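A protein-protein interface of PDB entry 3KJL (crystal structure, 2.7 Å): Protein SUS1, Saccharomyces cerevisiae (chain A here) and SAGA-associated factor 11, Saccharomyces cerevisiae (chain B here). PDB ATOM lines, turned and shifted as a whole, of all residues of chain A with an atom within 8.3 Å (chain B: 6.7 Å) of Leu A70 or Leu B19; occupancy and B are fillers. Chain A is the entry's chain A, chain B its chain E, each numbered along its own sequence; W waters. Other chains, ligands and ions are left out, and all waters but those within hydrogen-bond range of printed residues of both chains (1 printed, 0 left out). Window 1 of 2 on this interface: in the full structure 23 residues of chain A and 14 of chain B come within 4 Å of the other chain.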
ATOM      1  N   TYR A  22     -37.654  12.567 -36.210  1.00  0.00           N
ATOM      2  CA  TYR A  22     -36.929  12.143 -35.020  1.00  0.00           C
ATOM      3  C   TYR A  22     -35.795  11.226 -35.441  1.00  0.00           C
ATOM      4  O   TYR A  22     -34.666  11.362 -34.973  1.00  0.00           O
ATOM      5  CB  TYR A  22     -37.847  11.414 -34.040  1.00  0.00           C
ATOM      6  CG  TYR A  22     -37.174  11.086 -32.727  1.00  0.00           C
ATOM      7  CD1 TYR A  22     -37.512  11.761 -31.561  1.00  0.00           C
ATOM      8  CD2 TYR A  22     -36.183  10.115 -32.657  1.00  0.00           C
ATOM      9  CE1 TYR A  22     -36.894  11.467 -30.362  1.00  0.00           C
ATOM     10  CE2 TYR A  22     -35.559   9.817 -31.463  1.00  0.00           C
ATOM     11  CZ  TYR A  22     -35.918  10.496 -30.319  1.00  0.00           C
ATOM     12  OH  TYR A  22     -35.297  10.200 -29.128  1.00  0.00           O
ATOM     13  N   SER A  26     -31.707  11.778 -35.144  1.00  0.00           N
ATOM     14  CA  SER A  26     -30.799  10.786 -34.595  1.00  0.00           C
ATOM     15  C   SER A  26     -29.677  10.475 -35.580  1.00  0.00           C
ATOM     16  O   SER A  26     -28.553  10.198 -35.172  1.00  0.00           O
ATOM     17  CB  SER A  26     -31.559   9.507 -34.243  1.00  0.00           C
ATOM     18  OG  SER A  26     -30.699   8.559 -33.633  1.00  0.00           O
ATOM     19  N   LEU A  29     -27.047  13.576 -35.687  1.00  0.00           N
ATOM     20  CA  LEU A  29     -26.273  13.665 -34.454  1.00  0.00           C
ATOM     21  C   LEU A  29     -25.099  12.690 -34.488  1.00  0.00           C
ATOM     22  O   LEU A  29     -23.971  13.056 -34.164  1.00  0.00           O
ATOM     23  CB  LEU A  29     -27.160  13.390 -33.235  1.00  0.00           C
ATOM     24  CG  LEU A  29     -26.430  13.115 -31.915  1.00  0.00           C
ATOM     25  CD1 LEU A  29     -25.382  14.180 -31.623  1.00  0.00           C
ATOM     26  CD2 LEU A  29     -27.419  13.009 -30.762  1.00  0.00           C
ATOM     27  N   LYS A  30     -25.369  11.450 -34.890  1.00  0.00           N
ATOM     28  CA  LYS A  30     -24.331  10.427 -34.954  1.00  0.00           C
ATOM     29  C   LYS A  30     -23.212  10.851 -35.897  1.00  0.00           C
ATOM     30  O   LYS A  30     -22.056  10.475 -35.710  1.00  0.00           O
ATOM     31  CB  LYS A  30     -24.912   9.095 -35.426  1.00  0.00           C
ATOM     32  CG  LYS A  30     -25.985   8.514 -34.520  1.00  0.00           C
ATOM     33  CD  LYS A  30     -26.431   7.146 -35.016  1.00  0.00           C
ATOM     34  CE  LYS A  30     -27.735   6.700 -34.372  1.00  0.00           C
ATOM     35  NZ  LYS A  30     -28.109   5.319 -34.784  1.00  0.00           N
ATOM     36  N   LEU A  33     -20.738  13.595 -34.122  1.00  0.00           N
ATOM     37  CA  LEU A  33     -19.883  12.958 -33.133  1.00  0.00           C
ATOM     38  C   LEU A  33     -18.848  12.060 -33.805  1.00  0.00           C
ATOM     39  O   LEU A  33     -17.679  12.055 -33.427  1.00  0.00           O
ATOM     40  CB  LEU A  33     -20.731  12.145 -32.154  1.00  0.00           C
ATOM     41  CG  LEU A  33     -21.771  12.958 -31.382  1.00  0.00           C
ATOM     42  CD1 LEU A  33     -22.605  12.054 -30.489  1.00  0.00           C
ATOM     43  CD2 LEU A  33     -21.099  14.053 -30.571  1.00  0.00           C
ATOM     44  N   TRP A  38     -15.301  11.614 -31.871  1.00  0.00           N
ATOM     45  CA  TRP A  38     -15.845  11.477 -30.527  1.00  0.00           C
ATOM     46  C   TRP A  38     -16.126  10.015 -30.207  1.00  0.00           C
ATOM     47  O   TRP A  38     -15.910   9.565 -29.085  1.00  0.00           O
ATOM     48  CB  TRP A  38     -17.131  12.295 -30.395  1.00  0.00           C
ATOM     49  CG  TRP A  38     -17.808  12.155 -29.066  1.00  0.00           C
ATOM     50  CD1 TRP A  38     -17.551  12.873 -27.935  1.00  0.00           C
ATOM     51  CD2 TRP A  38     -18.859  11.241 -28.732  1.00  0.00           C
ATOM     52  NE1 TRP A  38     -18.376  12.463 -26.915  1.00  0.00           N
ATOM     53  CE2 TRP A  38     -19.190  11.460 -27.379  1.00  0.00           C
ATOM     54  CE3 TRP A  38     -19.552  10.256 -29.443  1.00  0.00           C
ATOM     55  CZ2 TRP A  38     -20.182  10.734 -26.724  1.00  0.00           C
ATOM     56  CZ3 TRP A  38     -20.538   9.535 -28.792  1.00  0.00           C
ATOM     57  CH2 TRP A  38     -20.842   9.778 -27.447  1.00  0.00           C
ATOM     58  N   VAL A  42     -14.540   7.544 -27.198  1.00  0.00           N
ATOM     59  CA  VAL A  42     -15.392   6.820 -26.264  1.00  0.00           C
ATOM     60  C   VAL A  42     -15.004   5.347 -26.217  1.00  0.00           C
ATOM     61  O   VAL A  42     -15.009   4.733 -25.152  1.00  0.00           O
ATOM     62  CB  VAL A  42     -16.882   6.946 -26.634  1.00  0.00           C
ATOM     63  CG1 VAL A  42     -17.707   5.885 -25.913  1.00  0.00           C
ATOM     64  CG2 VAL A  42     -17.387   8.341 -26.303  1.00  0.00           C
ATOM     65  N   LEU A  45     -12.126   5.093 -24.141  1.00  0.00           N
ATOM     66  CA  LEU A  45     -12.492   5.344 -22.753  1.00  0.00           C
ATOM     67  C   LEU A  45     -13.079   4.095 -22.104  1.00  0.00           C
ATOM     68  O   LEU A  45     -12.882   3.854 -20.914  1.00  0.00           O
ATOM     69  CB  LEU A  45     -13.491   6.501 -22.670  1.00  0.00           C
ATOM     70  CG  LEU A  45     -14.167   6.728 -21.315  1.00  0.00           C
ATOM     71  CD1 LEU A  45     -13.143   6.820 -20.191  1.00  0.00           C
ATOM     72  CD2 LEU A  45     -15.035   7.977 -21.360  1.00  0.00           C
ATOM     73  N   LEU A  62     -20.730   0.773 -17.626  1.00  0.00           N
ATOM     74  CA  LEU A  62     -21.569   1.825 -18.185  1.00  0.00           C
ATOM     75  C   LEU A  62     -21.639   3.034 -17.259  1.00  0.00           C
ATOM     76  O   LEU A  62     -21.700   4.173 -17.716  1.00  0.00           O
ATOM     77  CB  LEU A  62     -22.984   1.305 -18.443  1.00  0.00           C
ATOM     78  CG  LEU A  62     -23.947   2.330 -19.047  1.00  0.00           C
ATOM     79  CD1 LEU A  62     -23.566   2.643 -20.487  1.00  0.00           C
ATOM     80  CD2 LEU A  62     -25.381   1.833 -18.963  1.00  0.00           C
ATOM     81  N   VAL A  65     -18.270   5.121 -17.455  1.00  0.00           N
ATOM     82  CA  VAL A  65     -17.997   5.715 -18.759  1.00  0.00           C
ATOM     83  C   VAL A  65     -19.046   6.741 -19.186  1.00  0.00           C
ATOM     84  O   VAL A  65     -18.717   7.745 -19.814  1.00  0.00           O
ATOM     85  CB  VAL A  65     -17.907   4.625 -19.853  1.00  0.00           C
ATOM     86  CG1 VAL A  65     -17.971   5.247 -21.243  1.00  0.00           C
ATOM     87  CG2 VAL A  65     -16.639   3.805 -19.677  1.00  0.00           C
ATOM     88  N   GLU A  66     -20.304   6.486 -18.847  1.00  0.00           N
ATOM     89  CA  GLU A  66     -21.411   7.271 -19.387  1.00  0.00           C
ATOM     90  C   GLU A  66     -21.443   8.718 -18.889  1.00  0.00           C
ATOM     91  O   GLU A  66     -21.514   9.646 -19.694  1.00  0.00           O
ATOM     92  CB  GLU A  66     -22.743   6.583 -19.093  1.00  0.00           C
ATOM     93  CG  GLU A  66     -23.956   7.412 -19.457  1.00  0.00           C
ATOM     94  CD  GLU A  66     -25.183   6.558 -19.710  1.00  0.00           C
ATOM     95  OE1 GLU A  66     -25.055   5.531 -20.410  1.00  0.00           O
ATOM     96  OE2 GLU A  66     -26.275   6.911 -19.216  1.00  0.00           O
ATOM     97  N   PRO A  67     -21.401   8.914 -17.563  1.00  0.00           N
ATOM     98  CA  PRO A  67     -21.450  10.272 -17.007  1.00  0.00           C
ATOM     99  C   PRO A  67     -20.437  11.218 -17.645  1.00  0.00           C
ATOM    100  O   PRO A  67     -20.790  12.354 -17.957  1.00  0.00           O
ATOM    101  CB  PRO A  67     -21.125  10.053 -15.530  1.00  0.00           C
ATOM    102  CG  PRO A  67     -21.603   8.675 -15.250  1.00  0.00           C
ATOM    103  CD  PRO A  67     -21.359   7.891 -16.507  1.00  0.00           C
ATOM    104  N   LYS A  68     -19.204  10.759 -17.836  1.00  0.00           N
ATOM    105  CA  LYS A  68     -18.170  11.601 -18.427  1.00  0.00           C
ATOM    106  C   LYS A  68     -18.434  11.816 -19.914  1.00  0.00           C
ATOM    107  O   LYS A  68     -18.188  12.898 -20.445  1.00  0.00           O
ATOM    108  CB  LYS A  68     -16.784  10.981 -18.238  1.00  0.00           C
ATOM    109  CG  LYS A  68     -15.651  11.929 -18.592  1.00  0.00           C
ATOM    110  CD  LYS A  68     -14.308  11.224 -18.672  1.00  0.00           C
ATOM    111  CE  LYS A  68     -13.184  12.229 -18.869  1.00  0.00           C
ATOM    112  NZ  LYS A  68     -11.845  11.585 -18.934  1.00  0.00           N
ATOM    113  N   ALA A  69     -18.937  10.780 -20.576  1.00  0.00           N
ATOM    114  CA  ALA A  69     -19.183  10.831 -22.013  1.00  0.00           C
ATOM    115  C   ALA A  69     -20.211  11.901 -22.363  1.00  0.00           C
ATOM    116  O   ALA A  69     -20.108  12.556 -23.400  1.00  0.00           O
ATOM    117  CB  ALA A  69     -19.644   9.472 -22.516  1.00  0.00           C
ATOM    118  N   LEU A  70     -21.204  12.071 -21.497  1.00  0.00           N
ATOM    119  CA  LEU A  70     -22.226  13.088 -21.705  1.00  0.00           C
ATOM    120  C   LEU A  70     -21.594  14.470 -21.646  1.00  0.00           C
ATOM    121  O   LEU A  70     -22.011  15.388 -22.354  1.00  0.00           O
ATOM    122  CB  LEU A  70     -23.325  12.972 -20.647  1.00  0.00           C
ATOM    123  CG  LEU A  70     -24.179  11.705 -20.706  1.00  0.00           C
ATOM    124  CD1 LEU A  70     -25.109  11.632 -19.505  1.00  0.00           C
ATOM    125  CD2 LEU A  70     -24.967  11.646 -22.007  1.00  0.00           C
ATOM    126  N   GLU A  71     -20.579  14.608 -20.798  1.00  0.00           N
ATOM    127  CA  GLU A  71     -19.876  15.874 -20.642  1.00  0.00           C
ATOM    128  C   GLU A  71     -19.004  16.169 -21.856  1.00  0.00           C
ATOM    129  O   GLU A  71     -18.734  17.327 -22.167  1.00  0.00           O
ATOM    130  CB  GLU A  71     -18.998  15.845 -19.390  1.00  0.00           C
ATOM    131  CG  GLU A  71     -19.715  15.460 -18.102  1.00  0.00           C
ATOM    132  CD  GLU A  71     -20.507  16.606 -17.503  1.00  0.00           C
ATOM    133  OE1 GLU A  71     -21.129  17.369 -18.272  1.00  0.00           O
ATOM    134  OE2 GLU A  71     -20.510  16.742 -16.261  1.00  0.00           O
ATOM    135  N   MET A  72     -18.580  15.116 -22.548  1.00  0.00           N
ATOM    136  CA  MET A  72     -17.557  15.229 -23.584  1.00  0.00           C
ATOM    137  C   MET A  72     -18.053  15.791 -24.916  1.00  0.00           C
ATOM    138  O   MET A  72     -17.262  16.330 -25.690  1.00  0.00           O
ATOM    139  CB  MET A  72     -16.913  13.862 -23.827  1.00  0.00           C
ATOM    140  CG  MET A  72     -15.970  13.416 -22.721  1.00  0.00           C
ATOM    141  SD  MET A  72     -15.270  11.786 -23.035  1.00  0.00           S
ATOM    142  CE  MET A  72     -14.504  12.066 -24.628  1.00  0.00           C
ATOM    143  N   VAL A  73     -19.347  15.665 -25.191  1.00  0.00           N
ATOM    144  CA  VAL A  73     -19.880  16.081 -26.486  1.00  0.00           C
ATOM    145  C   VAL A  73     -19.485  17.528 -26.775  1.00  0.00           C
ATOM    146  O   VAL A  73     -19.573  18.389 -25.900  1.00  0.00           O
ATOM    147  CB  VAL A  73     -21.415  15.932 -26.557  1.00  0.00           C
ATOM    148  CG1 VAL A  73     -21.910  16.276 -27.953  1.00  0.00           C
ATOM    149  CG2 VAL A  73     -21.829  14.518 -26.176  1.00  0.00           C
ATOM    150  N   SER A  74     -19.041  17.784 -28.003  1.00  0.00           N
ATOM    151  CA  SER A  74     -18.539  19.102 -28.385  1.00  0.00           C
ATOM    152  C   SER A  74     -19.609  20.179 -28.245  1.00  0.00           C
ATOM    153  O   SER A  74     -20.804  19.883 -28.247  1.00  0.00           O
ATOM    154  CB  SER A  74     -18.015  19.074 -29.822  1.00  0.00           C
ATOM    155  OG  SER A  74     -19.054  18.789 -30.739  1.00  0.00           O
ATOM    156  N   THR A  77     -21.737  20.672 -31.546  1.00  0.00           N
ATOM    157  CA  THR A  77     -22.691  19.589 -31.771  1.00  0.00           C
ATOM    158  C   THR A  77     -23.966  19.803 -30.972  1.00  0.00           C
ATOM    159  O   THR A  77     -25.065  19.555 -31.465  1.00  0.00           O
ATOM    160  CB  THR A  77     -22.102  18.218 -31.385  1.00  0.00           C
ATOM    161  OG1 THR A  77     -21.057  17.870 -32.298  1.00  0.00           O
ATOM    162  CG2 THR A  77     -23.176  17.139 -31.420  1.00  0.00           C
ATOM    163  N   ARG A  78     -23.819  20.258 -29.733  1.00  0.00           N
ATOM    164  CA  ARG A  78     -24.971  20.486 -28.876  1.00  0.00           C
ATOM    165  C   ARG A  78     -25.913  21.509 -29.499  1.00  0.00           C
ATOM    166  O   ARG A  78     -27.092  21.236 -29.690  1.00  0.00           O
ATOM    167  CB  ARG A  78     -24.528  20.949 -27.488  1.00  0.00           C
ATOM    168  CG  ARG A  78     -23.965  19.832 -26.627  1.00  0.00           C
ATOM    169  CD  ARG A  78     -24.564  19.862 -25.231  1.00  0.00           C
ATOM    170  NE  ARG A  78     -24.456  18.568 -24.561  1.00  0.00           N
ATOM    171  CZ  ARG A  78     -25.346  18.099 -23.690  1.00  0.00           C
ATOM    172  NH1 ARG A  78     -26.420  18.815 -23.380  1.00  0.00           N
ATOM    173  NH2 ARG A  78     -25.165  16.910 -23.131  1.00  0.00           N
ATOM    174  N   VAL A  81     -27.590  20.392 -32.987  1.00  0.00           N
ATOM    175  CA  VAL A  81     -28.594  19.355 -32.791  1.00  0.00           C
ATOM    176  C   VAL A  81     -29.790  19.913 -32.032  1.00  0.00           C
ATOM    177  O   VAL A  81     -30.919  19.495 -32.259  1.00  0.00           O
ATOM    178  CB  VAL A  81     -28.025  18.141 -32.029  1.00  0.00           C
ATOM    179  CG1 VAL A  81     -29.152  17.259 -31.508  1.00  0.00           C
ATOM    180  CG2 VAL A  81     -27.092  17.347 -32.924  1.00  0.00           C
ATOM    181  N   LEU A  82     -29.540  20.859 -31.134  1.00  0.00           N
ATOM    182  CA  LEU A  82     -30.607  21.473 -30.352  1.00  0.00           C
ATOM    183  C   LEU A  82     -31.454  22.367 -31.249  1.00  0.00           C
ATOM    184  O   LEU A  82     -32.655  22.526 -31.031  1.00  0.00           O
ATOM    185  CB  LEU A  82     -30.028  22.290 -29.197  1.00  0.00           C
ATOM    186  CG  LEU A  82     -29.367  21.489 -28.073  1.00  0.00           C
ATOM    187  CD1 LEU A  82     -28.409  22.363 -27.279  1.00  0.00           C
ATOM    188  CD2 LEU A  82     -30.409  20.854 -27.161  1.00  0.00           C
ATOM    189  N   ILE A  85     -33.489  19.916 -33.196  1.00  0.00           N
ATOM    190  CA  ILE A  85     -34.501  19.371 -32.303  1.00  0.00           C
ATOM    191  C   ILE A  85     -35.590  20.414 -32.100  1.00  0.00           C
ATOM    192  O   ILE A  85     -36.739  20.078 -31.819  1.00  0.00           O
ATOM    193  CB  ILE A  85     -33.916  18.989 -30.928  1.00  0.00           C
ATOM    194  CG1 ILE A  85     -33.002  17.768 -31.046  1.00  0.00           C
ATOM    195  CG2 ILE A  85     -35.030  18.682 -29.940  1.00  0.00           C
ATOM    196  CD1 ILE A  85     -32.378  17.345 -29.728  1.00  0.00           C
ATOM    197  N   ASN B  12     -33.528  19.743 -24.850  1.00  0.00           N
ATOM    198  CA  ASN B  12     -32.264  19.271 -24.309  1.00  0.00           C
ATOM    199  C   ASN B  12     -32.383  17.838 -23.807  1.00  0.00           C
ATOM    200  O   ASN B  12     -31.466  17.034 -23.967  1.00  0.00           O
ATOM    201  CB  ASN B  12     -31.812  20.174 -23.164  1.00  0.00           C
ATOM    202  CG  ASN B  12     -30.410  19.858 -22.698  1.00  0.00           C
ATOM    203  OD1 ASN B  12     -29.436  20.104 -23.408  1.00  0.00           O
ATOM    204  ND2 ASN B  12     -30.300  19.295 -21.501  1.00  0.00           N
ATOM    205  N   ILE B  14     -34.478  15.409 -24.866  1.00  0.00           N
ATOM    206  CA  ILE B  14     -34.466  14.550 -26.045  1.00  0.00           C
ATOM    207  C   ILE B  14     -33.040  14.272 -26.503  1.00  0.00           C
ATOM    208  O   ILE B  14     -32.682  13.129 -26.784  1.00  0.00           O
ATOM    209  CB  ILE B  14     -35.227  15.196 -27.217  1.00  0.00           C
ATOM    210  CG1 ILE B  14     -36.725  15.255 -26.916  1.00  0.00           C
ATOM    211  CG2 ILE B  14     -34.981  14.420 -28.504  1.00  0.00           C
ATOM    212  CD1 ILE B  14     -37.528  15.952 -27.994  1.00  0.00           C
ATOM    213  N   LEU B  15     -32.234  15.326 -26.590  1.00  0.00           N
ATOM    214  CA  LEU B  15     -30.838  15.188 -26.979  1.00  0.00           C
ATOM    215  C   LEU B  15     -30.124  14.198 -26.068  1.00  0.00           C
ATOM    216  O   LEU B  15     -29.388  13.331 -26.534  1.00  0.00           O
ATOM    217  CB  LEU B  15     -30.128  16.542 -26.926  1.00  0.00           C
ATOM    218  CG  LEU B  15     -28.609  16.473 -27.113  1.00  0.00           C
ATOM    219  CD1 LEU B  15     -28.261  15.723 -28.388  1.00  0.00           C
ATOM    220  CD2 LEU B  15     -27.996  17.866 -27.116  1.00  0.00           C
ATOM    221  N   ASN B  16     -30.345  14.337 -24.764  1.00  0.00           N
ATOM    222  CA  ASN B  16     -29.713  13.471 -23.777  1.00  0.00           C
ATOM    223  C   ASN B  16     -30.084  11.999 -23.963  1.00  0.00           C
ATOM    224  O   ASN B  16     -29.291  11.117 -23.644  1.00  0.00           O
ATOM    225  CB  ASN B  16     -30.066  13.925 -22.357  1.00  0.00           C
ATOM    226  CG  ASN B  16     -29.262  15.134 -21.913  1.00  0.00           C
ATOM    227  OD1 ASN B  16     -28.187  15.412 -22.448  1.00  0.00           O
ATOM    228  ND2 ASN B  16     -29.776  15.852 -20.921  1.00  0.00           N
ATOM    229  N   ASN B  17     -31.282  11.732 -24.474  1.00  0.00           N
ATOM    230  CA  ASN B  17     -31.686  10.360 -24.775  1.00  0.00           C
ATOM    231  C   ASN B  17     -30.840   9.818 -25.913  1.00  0.00           C
ATOM    232  O   ASN B  17     -30.246   8.749 -25.809  1.00  0.00           O
ATOM    233  CB  ASN B  17     -33.159  10.291 -25.183  1.00  0.00           C
ATOM    234  CG  ASN B  17     -34.066  11.033 -24.232  1.00  0.00           C
ATOM    235  OD1 ASN B  17     -33.622  11.536 -23.202  1.00  0.00           O
ATOM    236  ND2 ASN B  17     -35.349  11.104 -24.571  1.00  0.00           N
ATOM    237  N   LEU B  18     -30.796  10.574 -27.005  1.00  0.00           N
ATOM    238  CA  LEU B  18     -30.041  10.192 -28.189  1.00  0.00           C
ATOM    239  C   LEU B  18     -28.585   9.935 -27.826  1.00  0.00           C
ATOM    240  O   LEU B  18     -27.925   9.084 -28.420  1.00  0.00           O
ATOM    241  CB  LEU B  18     -30.132  11.303 -29.235  1.00  0.00           C
ATOM    242  CG  LEU B  18     -31.562  11.720 -29.591  1.00  0.00           C
ATOM    243  CD1 LEU B  18     -31.576  12.950 -30.490  1.00  0.00           C
ATOM    244  CD2 LEU B  18     -32.309  10.561 -30.236  1.00  0.00           C
ATOM    245  N   LEU B  19     -28.090  10.678 -26.842  1.00  0.00           N
ATOM    246  CA  LEU B  19     -26.718  10.524 -26.382  1.00  0.00           C
ATOM    247  C   LEU B  19     -26.560   9.249 -25.562  1.00  0.00           C
ATOM    248  O   LEU B  19     -25.576   8.530 -25.710  1.00  0.00           O
ATOM    249  CB  LEU B  19     -26.296  11.731 -25.543  1.00  0.00           C
ATOM    250  CG  LEU B  19     -26.244  13.072 -26.277  1.00  0.00           C
ATOM    251  CD1 LEU B  19     -25.933  14.204 -25.307  1.00  0.00           C
ATOM    252  CD2 LEU B  19     -25.224  13.026 -27.404  1.00  0.00           C
ATOM    253  N   THR B  20     -27.531   8.971 -24.698  1.00  0.00           N
ATOM    254  CA  THR B  20     -27.466   7.792 -23.843  1.00  0.00           C
ATOM    255  C   THR B  20     -27.580   6.519 -24.677  1.00  0.00           C
ATOM    256  O   THR B  20     -26.998   5.494 -24.333  1.00  0.00           O
ATOM    257  CB  THR B  20     -28.571   7.803 -22.766  1.00  0.00           C
ATOM    258  OG1 THR B  20     -28.449   8.980 -21.958  1.00  0.00           O
ATOM    259  CG2 THR B  20     -28.450   6.584 -21.871  1.00  0.00           C
ATOM    260  N   THR B  21     -28.333   6.587 -25.772  1.00  0.00           N
ATOM    261  CA  THR B  21     -28.481   5.447 -26.667  1.00  0.00           C
ATOM    262  C   THR B  21     -27.130   5.102 -27.262  1.00  0.00           C
ATOM    263  O   THR B  21     -26.695   3.952 -27.228  1.00  0.00           O
ATOM    264  CB  THR B  21     -29.444   5.747 -27.833  1.00  0.00           C
ATOM    265  OG1 THR B  21     -30.752   6.048 -27.329  1.00  0.00           O
ATOM    266  CG2 THR B  21     -29.526   4.550 -28.779  1.00  0.00           C
ATOM    267  N   LEU B  22     -26.475   6.116 -27.811  1.00  0.00           N
ATOM    268  CA  LEU B  22     -25.190   5.942 -28.469  1.00  0.00           C
ATOM    269  C   LEU B  22     -24.117   5.484 -27.487  1.00  0.00           C
ATOM    270  O   LEU B  22     -23.298   4.631 -27.817  1.00  0.00           O
ATOM    271  CB  LEU B  22     -24.768   7.249 -29.138  1.00  0.00           C
ATOM    272  CG  LEU B  22     -25.763   7.756 -30.184  1.00  0.00           C
ATOM    273  CD1 LEU B  22     -25.335   9.100 -30.751  1.00  0.00           C
ATOM    274  CD2 LEU B  22     -25.942   6.731 -31.293  1.00  0.00           C
ATOM    275  N   ILE B  23     -24.127   6.044 -26.283  1.00  0.00           N
ATOM    276  CA  ILE B  23     -23.154   5.664 -25.266  1.00  0.00           C
ATOM    277  C   ILE B  23     -23.343   4.199 -24.877  1.00  0.00           C
ATOM    278  O   ILE B  23     -22.372   3.481 -24.649  1.00  0.00           O
ATOM    279  CB  ILE B  23     -23.273   6.544 -24.008  1.00  0.00           C
ATOM    280  CG1 ILE B  23     -22.895   7.991 -24.331  1.00  0.00           C
ATOM    281  CG2 ILE B  23     -22.380   6.008 -22.901  1.00  0.00           C
ATOM    282  CD1 ILE B  23     -23.048   8.935 -23.156  1.00  0.00           C
ATOM    283  N   GLN B  24     -24.597   3.766 -24.806  1.00  0.00           N
ATOM    284  CA  GLN B  24     -24.922   2.388 -24.455  1.00  0.00           C
ATOM    285  C   GLN B  24     -24.486   1.434 -25.559  1.00  0.00           C
ATOM    286  O   GLN B  24     -23.994   0.342 -25.290  1.00  0.00           O
ATOM    287  CB  GLN B  24     -26.427   2.231 -24.226  1.00  0.00           C
ATOM    288  CG  GLN B  24     -26.957   2.922 -22.980  1.00  0.00           C
ATOM    289  CD  GLN B  24     -28.477   2.949 -22.919  1.00  0.00           C
ATOM    290  OE1 GLN B  24     -29.058   3.704 -22.143  1.00  0.00           O
ATOM    291  NE2 GLN B  24     -29.127   2.130 -23.738  1.00  0.00           N
HETATM  292  O   HOH W   1     -27.461   4.465 -20.139  1.00  0.00           O
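The guanidinium group (NH1) of Arg A78 sits at hydrogen-bond distance from the side-chain amide oxygen (OD1) of Asn B12 (3.3 Å). The side-chain amide oxygen of Asn B16 is in hydrogen-bond range of the guanidinium group of Arg A78 (3.4 Å).
The backbone carbonyl oxygen (O) of Asn B16 is in hydrogen-bond range of the side-chain hydroxyl (OG1) of Thr B20 (2.8 Å). OE1 of Gln B24 lies close to O of Thr B20, at 3.5 Å.
Leu B15 touches Leu A29. Leu B18 touches Leu A29 (CB to CD2, 3.6 Å). Lys A30 touches Leu B22 (CE to CD2, 3.6 Å). OE2 of Glu A66 touches CG2 of Thr B20 (3.4 Å). Ile B23 touches Ala A69. CD2 of Leu A70 touches CD1 of Ile B23 (3.5 Å). Leu B19 touches Val A73. NH2 of Arg A78 touches CD1 of Leu B19, at 3.6 Å. Leu A82 touches Leu B15 (CD2 to CD2, 3.8 Å). CD1 of Ile A85 touches CB of Leu B15, at 3.7 Å.
Leu A33 touches none of the printed residues of chain B. Of chain B, only Leu B19 (3.8 Å) and Ile B23 (3.5 Å) come within 4 Å of Leu A70. Printed residues of chain A within 4 Å of Asn B12: Arg A78 and Leu A82. Of the printed residues of chain A, Leu B18 touches Tyr A22 (3.2 Å) and Leu A29 (3.6 Å). Printed residues of chain A within 4 Å of Leu B19: Leu A70 (3.8 Å), Val A73 (3.9 Å) and Arg A78 (3.6 Å). The nearest printed residue of chain A that does not touch Leu B19 is Leu A29 (4.01 Å).
Of the 12 printed residues of chain B, 9 touch a printed residue of chain A. Of the 24 printed residues of chain A, 11 touch a printed residue of chain B. Hydrophobic or aromatic side chains of chain A that line the printed part of chain B: Tyr A22, Leu A29, Ala A69, Leu A70, Val A73, Val A81, Leu A82 and Ile A85.
Water W1 bridges OE1 of Glu A66 and OE1 of Gln B24.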
